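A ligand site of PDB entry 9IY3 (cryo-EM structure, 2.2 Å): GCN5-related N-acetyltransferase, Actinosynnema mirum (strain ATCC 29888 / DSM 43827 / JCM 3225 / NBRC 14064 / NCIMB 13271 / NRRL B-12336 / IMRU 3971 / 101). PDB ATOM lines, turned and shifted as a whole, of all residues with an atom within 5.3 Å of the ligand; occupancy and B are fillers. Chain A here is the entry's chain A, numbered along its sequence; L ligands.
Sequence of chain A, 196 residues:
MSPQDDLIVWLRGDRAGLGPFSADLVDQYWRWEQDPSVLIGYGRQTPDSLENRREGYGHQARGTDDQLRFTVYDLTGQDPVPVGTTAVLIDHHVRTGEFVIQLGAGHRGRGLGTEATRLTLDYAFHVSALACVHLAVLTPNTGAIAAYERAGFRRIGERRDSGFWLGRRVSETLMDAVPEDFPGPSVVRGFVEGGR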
ATOM      1  N   ARG A  15       0.345  21.880  31.377  1.00  0.00           N
ATOM      2  CA  ARG A  15       1.434  21.167  30.736  1.00  0.00           C
ATOM      3  C   ARG A  15       2.481  20.624  31.703  1.00  0.00           C
ATOM      4  O   ARG A  15       3.140  19.639  31.368  1.00  0.00           O
ATOM      5  CB  ARG A  15       2.140  22.067  29.717  1.00  0.00           C
ATOM      6  CG  ARG A  15       1.242  22.552  28.583  1.00  0.00           C
ATOM      7  CD  ARG A  15       1.005  21.450  27.569  1.00  0.00           C
ATOM      8  NE  ARG A  15       2.253  20.966  27.011  1.00  0.00           N
ATOM      9  CZ  ARG A  15       2.918  21.566  26.032  1.00  0.00           C
ATOM     10  NH1 ARG A  15       2.486  22.696  25.485  1.00  0.00           N
ATOM     11  NH2 ARG A  15       4.061  21.028  25.597  1.00  0.00           N
ATOM     12  N   SER A  37      25.185  22.813  28.383  1.00  0.00           N
ATOM     13  CA  SER A  37      24.241  23.903  28.161  1.00  0.00           C
ATOM     14  C   SER A  37      23.796  24.529  29.472  1.00  0.00           C
ATOM     15  O   SER A  37      23.692  25.760  29.574  1.00  0.00           O
ATOM     16  CB  SER A  37      23.038  23.395  27.364  1.00  0.00           C
ATOM     17  OG  SER A  37      23.402  23.029  26.053  1.00  0.00           O
ATOM     18  N   VAL A  38      23.522  23.703  30.485  1.00  0.00           N
ATOM     19  CA  VAL A  38      23.136  24.234  31.791  1.00  0.00           C
ATOM     20  C   VAL A  38      24.290  24.998  32.431  1.00  0.00           C
ATOM     21  O   VAL A  38      24.093  26.036  33.055  1.00  0.00           O
ATOM     22  CB  VAL A  38      22.631  23.101  32.698  1.00  0.00           C
ATOM     23  CG1 VAL A  38      22.375  23.614  34.098  1.00  0.00           C
ATOM     24  CG2 VAL A  38      21.385  22.481  32.114  1.00  0.00           C
ATOM     25  N   GLY A  41      24.440  28.337  30.680  1.00  0.00           N
ATOM     26  CA  GLY A  41      23.336  29.210  31.065  1.00  0.00           C
ATOM     27  C   GLY A  41      23.481  29.765  32.473  1.00  0.00           C
ATOM     28  O   GLY A  41      23.296  30.954  32.698  1.00  0.00           O
ATOM     29  N   TYR A  42      23.822  28.894  33.431  1.00  0.00           N
ATOM     30  CA  TYR A  42      24.027  29.350  34.799  1.00  0.00           C
ATOM     31  C   TYR A  42      25.279  30.208  34.923  1.00  0.00           C
ATOM     32  O   TYR A  42      25.328  31.116  35.768  1.00  0.00           O
ATOM     33  CB  TYR A  42      24.115  28.170  35.765  1.00  0.00           C
ATOM     34  CG  TYR A  42      22.795  27.574  36.164  1.00  0.00           C
ATOM     35  CD1 TYR A  42      21.619  27.910  35.497  1.00  0.00           C
ATOM     36  CD2 TYR A  42      22.704  26.673  37.216  1.00  0.00           C
ATOM     37  CE1 TYR A  42      20.408  27.364  35.871  1.00  0.00           C
ATOM     38  CE2 TYR A  42      21.509  26.127  37.597  1.00  0.00           C
ATOM     39  CZ  TYR A  42      20.352  26.475  36.918  1.00  0.00           C
ATOM     40  OH  TYR A  42      19.153  25.922  37.294  1.00  0.00           O
ATOM     41  N   ILE A 101      16.121  28.009  37.593  1.00  0.00           N
ATOM     42  CA  ILE A 101      15.410  26.919  36.936  1.00  0.00           C
ATOM     43  C   ILE A 101      16.314  26.321  35.874  1.00  0.00           C
ATOM     44  O   ILE A 101      17.094  27.028  35.226  1.00  0.00           O
ATOM     45  CB  ILE A 101      14.074  27.410  36.327  1.00  0.00           C
ATOM     46  CG1 ILE A 101      13.357  26.284  35.592  1.00  0.00           C
ATOM     47  CG2 ILE A 101      14.312  28.579  35.388  1.00  0.00           C
ATOM     48  CD1 ILE A 101      11.939  26.587  35.203  1.00  0.00           C
ATOM     49  N   GLN A 102      16.206  25.006  35.696  1.00  0.00           N
ATOM     50  CA  GLN A 102      16.847  24.314  34.592  1.00  0.00           C
ATOM     51  C   GLN A 102      16.011  23.102  34.226  1.00  0.00           C
ATOM     52  O   GLN A 102      15.388  22.481  35.087  1.00  0.00           O
ATOM     53  CB  GLN A 102      18.298  23.918  34.917  1.00  0.00           C
ATOM     54  CG  GLN A 102      18.453  22.932  36.070  1.00  0.00           C
ATOM     55  CD  GLN A 102      18.288  21.494  35.634  1.00  0.00           C
ATOM     56  OE1 GLN A 102      18.583  21.140  34.492  1.00  0.00           O
ATOM     57  NE2 GLN A 102      17.814  20.651  36.542  1.00  0.00           N
ATOM     58  N   LEU A 103      16.003  22.775  32.941  1.00  0.00           N
ATOM     59  CA  LEU A 103      15.327  21.591  32.428  1.00  0.00           C
ATOM     60  C   LEU A 103      16.330  20.647  31.784  1.00  0.00           C
ATOM     61  O   LEU A 103      17.490  20.989  31.550  1.00  0.00           O
ATOM     62  CB  LEU A 103      14.226  21.948  31.425  1.00  0.00           C
ATOM     63  CG  LEU A 103      13.126  22.906  31.878  1.00  0.00           C
ATOM     64  CD1 LEU A 103      12.185  23.198  30.726  1.00  0.00           C
ATOM     65  CD2 LEU A 103      12.363  22.329  33.053  1.00  0.00           C
ATOM     66  N   GLY A 104      15.859  19.441  31.485  1.00  0.00           N
ATOM     67  CA  GLY A 104      16.690  18.459  30.820  1.00  0.00           C
ATOM     68  C   GLY A 104      16.960  18.829  29.371  1.00  0.00           C
ATOM     69  O   GLY A 104      16.332  19.706  28.784  1.00  0.00           O
ATOM     70  N   HIS A 107      13.949  18.156  26.979  1.00  0.00           N
ATOM     71  CA  HIS A 107      12.669  18.697  27.385  1.00  0.00           C
ATOM     72  C   HIS A 107      12.538  20.199  27.138  1.00  0.00           C
ATOM     73  O   HIS A 107      11.546  20.801  27.556  1.00  0.00           O
ATOM     74  CB  HIS A 107      12.432  18.401  28.874  1.00  0.00           C
ATOM     75  CG  HIS A 107      12.585  16.950  29.221  1.00  0.00           C
ATOM     76  ND1 HIS A 107      11.730  15.984  28.747  1.00  0.00           N
ATOM     77  CD2 HIS A 107      13.499  16.306  29.977  1.00  0.00           C
ATOM     78  CE1 HIS A 107      12.104  14.799  29.210  1.00  0.00           C
ATOM     79  NE2 HIS A 107      13.179  14.972  29.954  1.00  0.00           N
ATOM     80  N   ARG A 108      13.504  20.811  26.462  1.00  0.00           N
ATOM     81  CA  ARG A 108      13.481  22.244  26.210  1.00  0.00           C
ATOM     82  C   ARG A 108      12.793  22.539  24.895  1.00  0.00           C
ATOM     83  O   ARG A 108      12.762  21.701  23.974  1.00  0.00           O
ATOM     84  CB  ARG A 108      14.909  22.797  26.193  1.00  0.00           C
ATOM     85  CG  ARG A 108      15.662  22.576  27.486  1.00  0.00           C
ATOM     86  CD  ARG A 108      17.153  22.729  27.280  1.00  0.00           C
ATOM     87  NE  ARG A 108      17.911  22.207  28.406  1.00  0.00           N
ATOM     88  CZ  ARG A 108      19.190  21.873  28.356  1.00  0.00           C
ATOM     89  NH1 ARG A 108      19.893  21.988  27.237  1.00  0.00           N
ATOM     90  NH2 ARG A 108      19.788  21.396  29.448  1.00  0.00           N
ATOM     91  N   GLY A 109      12.232  23.739  24.789  1.00  0.00           N
ATOM     92  CA  GLY A 109      11.544  24.158  23.583  1.00  0.00           C
ATOM     93  C   GLY A 109      10.117  23.677  23.459  1.00  0.00           C
ATOM     94  O   GLY A 109       9.448  24.003  22.467  1.00  0.00           O
ATOM     95  N   ARG A 110       9.631  22.889  24.413  1.00  0.00           N
ATOM     96  CA  ARG A 110       8.256  22.419  24.424  1.00  0.00           C
ATOM     97  C   ARG A 110       7.344  23.256  25.304  1.00  0.00           C
ATOM     98  O   ARG A 110       6.160  22.926  25.442  1.00  0.00           O
ATOM     99  CB  ARG A 110       8.210  20.951  24.874  1.00  0.00           C
ATOM    100  CG  ARG A 110       8.773  19.986  23.841  1.00  0.00           C
ATOM    101  CD  ARG A 110       9.240  18.686  24.471  1.00  0.00           C
ATOM    102  NE  ARG A 110       8.176  18.036  25.222  1.00  0.00           N
ATOM    103  CZ  ARG A 110       8.361  17.048  26.086  1.00  0.00           C
ATOM    104  NH1 ARG A 110       9.571  16.577  26.344  1.00  0.00           N
ATOM    105  NH2 ARG A 110       7.315  16.512  26.700  1.00  0.00           N
ATOM    106  N   GLY A 111       7.861  24.333  25.902  1.00  0.00           N
ATOM    107  CA  GLY A 111       7.082  25.222  26.718  1.00  0.00           C
ATOM    108  C   GLY A 111       7.107  24.929  28.207  1.00  0.00           C
ATOM    109  O   GLY A 111       6.679  25.785  28.984  1.00  0.00           O
ATOM    110  N   LEU A 112       7.627  23.768  28.616  1.00  0.00           N
ATOM    111  CA  LEU A 112       7.512  23.345  30.019  1.00  0.00           C
ATOM    112  C   LEU A 112       8.141  24.354  30.972  1.00  0.00           C
ATOM    113  O   LEU A 112       7.683  24.487  32.117  1.00  0.00           O
ATOM    114  CB  LEU A 112       8.158  21.971  30.193  1.00  0.00           C
ATOM    115  CG  LEU A 112       7.509  20.807  29.459  1.00  0.00           C
ATOM    116  CD1 LEU A 112       8.390  19.578  29.547  1.00  0.00           C
ATOM    117  CD2 LEU A 112       6.127  20.514  30.027  1.00  0.00           C
ATOM    118  N   GLY A 113       9.185  25.050  30.534  1.00  0.00           N
ATOM    119  CA  GLY A 113       9.836  26.015  31.416  1.00  0.00           C
ATOM    120  C   GLY A 113       8.935  27.171  31.794  1.00  0.00           C
ATOM    121  O   GLY A 113       8.968  27.646  32.926  1.00  0.00           O
ATOM    122  N   THR A 114       8.096  27.622  30.851  1.00  0.00           N
ATOM    123  CA  THR A 114       7.215  28.753  31.133  1.00  0.00           C
ATOM    124  C   THR A 114       6.215  28.413  32.233  1.00  0.00           C
ATOM    125  O   THR A 114       6.084  29.150  33.215  1.00  0.00           O
ATOM    126  CB  THR A 114       6.482  29.181  29.855  1.00  0.00           C
ATOM    127  OG1 THR A 114       7.450  29.555  28.865  1.00  0.00           O
ATOM    128  CG2 THR A 114       5.570  30.356  30.136  1.00  0.00           C
ATOM    129  N   ALA A 136      18.788  36.672  38.173  1.00  0.00           N
ATOM    130  CA  ALA A 136      19.845  37.227  37.332  1.00  0.00           C
ATOM    131  C   ALA A 136      20.164  36.223  36.240  1.00  0.00           C
ATOM    132  O   ALA A 136      20.493  35.059  36.536  1.00  0.00           O
ATOM    133  CB  ALA A 136      21.091  37.564  38.148  1.00  0.00           C
ATOM    134  N   VAL A 137      20.091  36.655  34.991  1.00  0.00           N
ATOM    135  CA  VAL A 137      20.279  35.792  33.838  1.00  0.00           C
ATOM    136  C   VAL A 137      21.154  36.508  32.816  1.00  0.00           C
ATOM    137  O   VAL A 137      21.035  37.716  32.617  1.00  0.00           O
ATOM    138  CB  VAL A 137      18.930  35.352  33.231  1.00  0.00           C
ATOM    139  CG1 VAL A 137      18.181  36.551  32.681  1.00  0.00           C
ATOM    140  CG2 VAL A 137      19.141  34.324  32.143  1.00  0.00           C
ATOM    141  N   ASN A 141      21.323  34.783  26.749  1.00  0.00           N
ATOM    142  CA  ASN A 141      20.370  33.698  26.963  1.00  0.00           C
ATOM    143  C   ASN A 141      18.953  34.229  26.725  1.00  0.00           C
ATOM    144  O   ASN A 141      18.156  34.439  27.644  1.00  0.00           O
ATOM    145  CB  ASN A 141      20.521  33.121  28.359  1.00  0.00           C
ATOM    146  CG  ASN A 141      19.790  31.811  28.548  1.00  0.00           C
ATOM    147  OD1 ASN A 141      18.894  31.464  27.777  1.00  0.00           O
ATOM    148  ND2 ASN A 141      20.164  31.059  29.576  1.00  0.00           N
ATOM    149  N   GLY A 143      16.353  32.868  25.147  1.00  0.00           N
ATOM    150  CA  GLY A 143      15.253  31.956  25.401  1.00  0.00           C
ATOM    151  C   GLY A 143      14.759  32.028  26.836  1.00  0.00           C
ATOM    152  O   GLY A 143      13.561  32.060  27.099  1.00  0.00           O
ATOM    153  N   ALA A 144      15.700  32.064  27.785  1.00  0.00           N
ATOM    154  CA  ALA A 144      15.326  32.240  29.186  1.00  0.00           C
ATOM    155  C   ALA A 144      14.659  33.585  29.414  1.00  0.00           C
ATOM    156  O   ALA A 144      13.721  33.697  30.221  1.00  0.00           O
ATOM    157  CB  ALA A 144      16.549  32.089  30.085  1.00  0.00           C
ATOM    158  N   ALA A 146      12.743  35.238  27.256  1.00  0.00           N
ATOM    159  CA  ALA A 146      11.362  35.120  26.790  1.00  0.00           C
ATOM    160  C   ALA A 146      10.526  34.282  27.745  1.00  0.00           C
ATOM    161  O   ALA A 146       9.363  34.614  28.032  1.00  0.00           O
ATOM    162  CB  ALA A 146      11.334  34.525  25.385  1.00  0.00           C
ATOM    163  N   ALA A 147      11.089  33.179  28.248  1.00  0.00           N
ATOM    164  CA  ALA A 147      10.363  32.328  29.192  1.00  0.00           C
ATOM    165  C   ALA A 147       9.996  33.095  30.451  1.00  0.00           C
ATOM    166  O   ALA A 147       8.869  32.998  30.940  1.00  0.00           O
ATOM    167  CB  ALA A 147      11.199  31.098  29.528  1.00  0.00           C
ATOM    168  N   TYR A 148      10.938  33.866  31.000  1.00  0.00           N
ATOM    169  CA  TYR A 148      10.671  34.625  32.212  1.00  0.00           C
ATOM    170  C   TYR A 148       9.656  35.742  31.949  1.00  0.00           C
ATOM    171  O   TYR A 148       8.799  36.018  32.801  1.00  0.00           O
ATOM    172  CB  TYR A 148      11.960  35.191  32.780  1.00  0.00           C
ATOM    173  CG  TYR A 148      12.985  34.133  33.142  1.00  0.00           C
ATOM    174  CD1 TYR A 148      12.588  32.844  33.460  1.00  0.00           C
ATOM    175  CD2 TYR A 148      14.337  34.420  33.143  1.00  0.00           C
ATOM    176  CE1 TYR A 148      13.524  31.878  33.779  1.00  0.00           C
ATOM    177  CE2 TYR A 148      15.273  33.468  33.461  1.00  0.00           C
ATOM    178  CZ  TYR A 148      14.865  32.186  33.777  1.00  0.00           C
ATOM    179  OH  TYR A 148      15.793  31.235  34.101  1.00  0.00           O
ATOM    180  N   ARG A 150       7.209  35.776  29.672  1.00  0.00           N
ATOM    181  CA  ARG A 150       5.868  35.194  29.568  1.00  0.00           C
ATOM    182  C   ARG A 150       5.407  34.591  30.888  1.00  0.00           C
ATOM    183  O   ARG A 150       4.198  34.494  31.135  1.00  0.00           O
ATOM    184  CB  ARG A 150       5.806  34.166  28.445  1.00  0.00           C
ATOM    185  CG  ARG A 150       5.938  34.755  27.060  1.00  0.00           C
ATOM    186  CD  ARG A 150       5.663  33.739  25.973  1.00  0.00           C
ATOM    187  NE  ARG A 150       6.639  32.646  25.964  1.00  0.00           N
ATOM    188  CZ  ARG A 150       7.768  32.675  25.285  1.00  0.00           C
ATOM    189  NH1 ARG A 150       8.114  33.718  24.554  1.00  0.00           N
ATOM    190  NH2 ARG A 150       8.586  31.623  25.341  1.00  0.00           N
HETATM  191  N1  LIG L   1       3.826  24.074  22.749  1.00  0.00           N
HETATM  192  C1  LIG L   1       5.120  23.844  22.538  1.00  0.00           C
HETATM  193  N2  LIG L   1       5.990  24.797  22.328  1.00  0.00           N
HETATM  194  C2  LIG L   1       5.615  26.070  22.315  1.00  0.00           C
HETATM  195  C3  LIG L   1       4.254  26.366  22.522  1.00  0.00           C
HETATM  196  C4  LIG L   1       3.360  25.323  22.746  1.00  0.00           C
HETATM  197  N3  LIG L   1       2.013  25.577  22.963  1.00  0.00           N
HETATM  198  N4  LIG L   1       4.121  27.710  22.466  1.00  0.00           N
HETATM  199  C5  LIG L   1       5.288  28.251  22.229  1.00  0.00           C
HETATM  200  N5  LIG L   1       6.236  27.284  22.120  1.00  0.00           N
HETATM  201  C6  LIG L   1       7.652  27.536  21.871  1.00  0.00           C
HETATM  202  C7  LIG L   1       7.967  28.980  22.353  1.00  0.00           C
HETATM  203  O1  LIG L   1       7.920  29.882  21.254  1.00  0.00           O
HETATM  204  C8  LIG L   1       9.408  28.864  22.916  1.00  0.00           C
HETATM  205  O2  LIG L   1      10.387  29.202  21.931  1.00  0.00           O
HETATM  206  P1  LIG L   1      11.089  30.536  22.459  1.00  0.00           P
HETATM  207  O3  LIG L   1      12.376  30.733  21.757  1.00  0.00           O
HETATM  208  O4  LIG L   1      10.113  31.790  22.161  1.00  0.00           O
HETATM  209  O5  LIG L   1      11.344  30.399  24.041  1.00  0.00           O
HETATM  210  C9  LIG L   1       9.511  27.372  23.323  1.00  0.00           C
HETATM  211  O6  LIG L   1       8.461  26.652  22.671  1.00  0.00           O
HETATM  212  C10 LIG L   1       9.338  27.259  24.826  1.00  0.00           C
HETATM  213  O7  LIG L   1      10.583  27.321  25.519  1.00  0.00           O
HETATM  214  P2  LIG L   1      10.248  28.225  26.806  1.00  0.00           P
HETATM  215  O8  LIG L   1       9.266  27.525  27.659  1.00  0.00           O
HETATM  216  O9  LIG L   1       9.612  29.587  26.238  1.00  0.00           O
HETATM  217  O10 LIG L   1      11.572  28.609  27.626  1.00  0.00           O
HETATM  218  P3  LIG L   1      12.369  27.305  28.137  1.00  0.00           P
HETATM  219  O11 LIG L   1      13.456  27.044  27.177  1.00  0.00           O
HETATM  220  O12 LIG L   1      11.414  26.009  28.233  1.00  0.00           O
HETATM  221  O13 LIG L   1      12.994  27.617  29.590  1.00  0.00           O
HETATM  222  C11 LIG L   1      15.141  26.755  30.225  1.00  0.00           C
HETATM  223  C12 LIG L   1      13.662  26.434  30.048  1.00  0.00           C
HETATM  224  C13 LIG L   1      15.508  26.604  31.703  1.00  0.00           C
HETATM  225  C14 LIG L   1      15.398  28.202  29.793  1.00  0.00           C
HETATM  226  C15 LIG L   1      15.935  25.808  29.329  1.00  0.00           C
HETATM  227  O14 LIG L   1      16.116  26.397  28.039  1.00  0.00           O
HETATM  228  C16 LIG L   1      17.290  25.462  29.905  1.00  0.00           C
HETATM  229  O15 LIG L   1      17.451  24.393  30.445  1.00  0.00           O
HETATM  230  N6  LIG L   1      18.326  26.315  29.823  1.00  0.00           N
HETATM  231  C17 LIG L   1      19.624  25.942  30.388  1.00  0.00           C
HETATM  232  C18 LIG L   1      19.691  26.358  31.865  1.00  0.00           C
HETATM  233  C19 LIG L   1      19.395  27.832  31.980  1.00  0.00           C
HETATM  234  O16 LIG L   1      19.653  28.568  31.051  1.00  0.00           O
HETATM  235  N7  LIG L   1      18.840  28.316  33.103  1.00  0.00           N
HETATM  236  C20 LIG L   1      18.545  29.742  33.229  1.00  0.00           C
HETATM  237  C21 LIG L   1      19.745  30.465  33.835  1.00  0.00           C
HETATM  238  S1  LIG L   1      19.149  31.887  34.797  1.00  0.00           S
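O9 of the ligand is in salt-bridge range of NH2 of Arg 150.
O16 of the ligand sits at hydrogen-bond distance from ND2 of Asn 141, at 2.9 Å.
The backbone NH (N) of Thr 114 lies within hydrogen-bond range of an oxygen (O8) of the ligand, 3.4 Å away.
An oxygen (O8) of the ligand is in hydrogen-bond range of the side-chain hydroxyl of Thr 114.
The guanidinium group (NE) of Arg 108 sits at hydrogen-bond distance from an oxygen (O15) of the ligand.
O of Ile 101 is in hydrogen-bond range of N7 of the ligand, 3.0 Å away.
S1 of the ligand sits close to OH of Tyr 148 (3.5 Å).
N of Leu 103 sits at hydrogen-bond distance from O15 of the ligand (3.3 Å).
An oxygen (O12) of the ligand sits at hydrogen-bond distance from the backbone NH of Gly 113 (3.3 Å).
The guanidinium group of Arg 15 sits at hydrogen-bond distance from a nitrogen (N1) of the ligand (3.3 Å).
N of Ala 144 sits at hydrogen-bond distance from OD1 of Asn 141.
The guanidinium group (NH2) of Arg 108 lies within hydrogen-bond range of the backbone carbonyl oxygen (O) of Leu 103 (3.1 Å).
The guanidinium group of Arg 108 is in hydrogen-bond range of the backbone carbonyl oxygen of Gly 104.
The side-chain hydroxyl (OH) of Tyr 42 sits at hydrogen-bond distance from the backbone carbonyl oxygen (O) of Ile 101 (3.1 Å).
NH2 of Arg 15 is in hydrogen-bond range of O of Arg 110 (2.8 Å).
The guanidinium group (NH1) of Arg 110 is in hydrogen-bond range of a ring nitrogen (ND1) of His 107 (3.3 Å).
The side-chain hydroxyl (OH) of Tyr 42 lies close to the backbone NH (N) of Gln 102 (3.5 Å).
The backbone carbonyl oxygen (O) of Gly 109 lies close to an oxygen (O6) of the ligand (2.8 Å).
O of Gly 111 lies close to O8 of the ligand (3.4 Å).
Residues that only touch the ligand: Ala 147 (3.2 Å), Arg 110 (3.2 Å), Tyr 42 (3.3 Å), Val 137 (3.6 Å), Gly 41 (3.7 Å), Ala 136 (3.9 Å) and Gln 102 (3.9 Å).
Within 4 Å of the ligand: Arg 15, Gly 41, Tyr 42, Ile 101, Gln 102, Leu 103, Arg 108, Gly 109, Arg 110, Gly 111, Gly 113, Thr 114, Ala 136, Val 137, Asn 141, Ala 147, Tyr 148 and Arg 150.
The nearest printed residue that does not touch the ligand is Gly 143 (4.02 Å).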
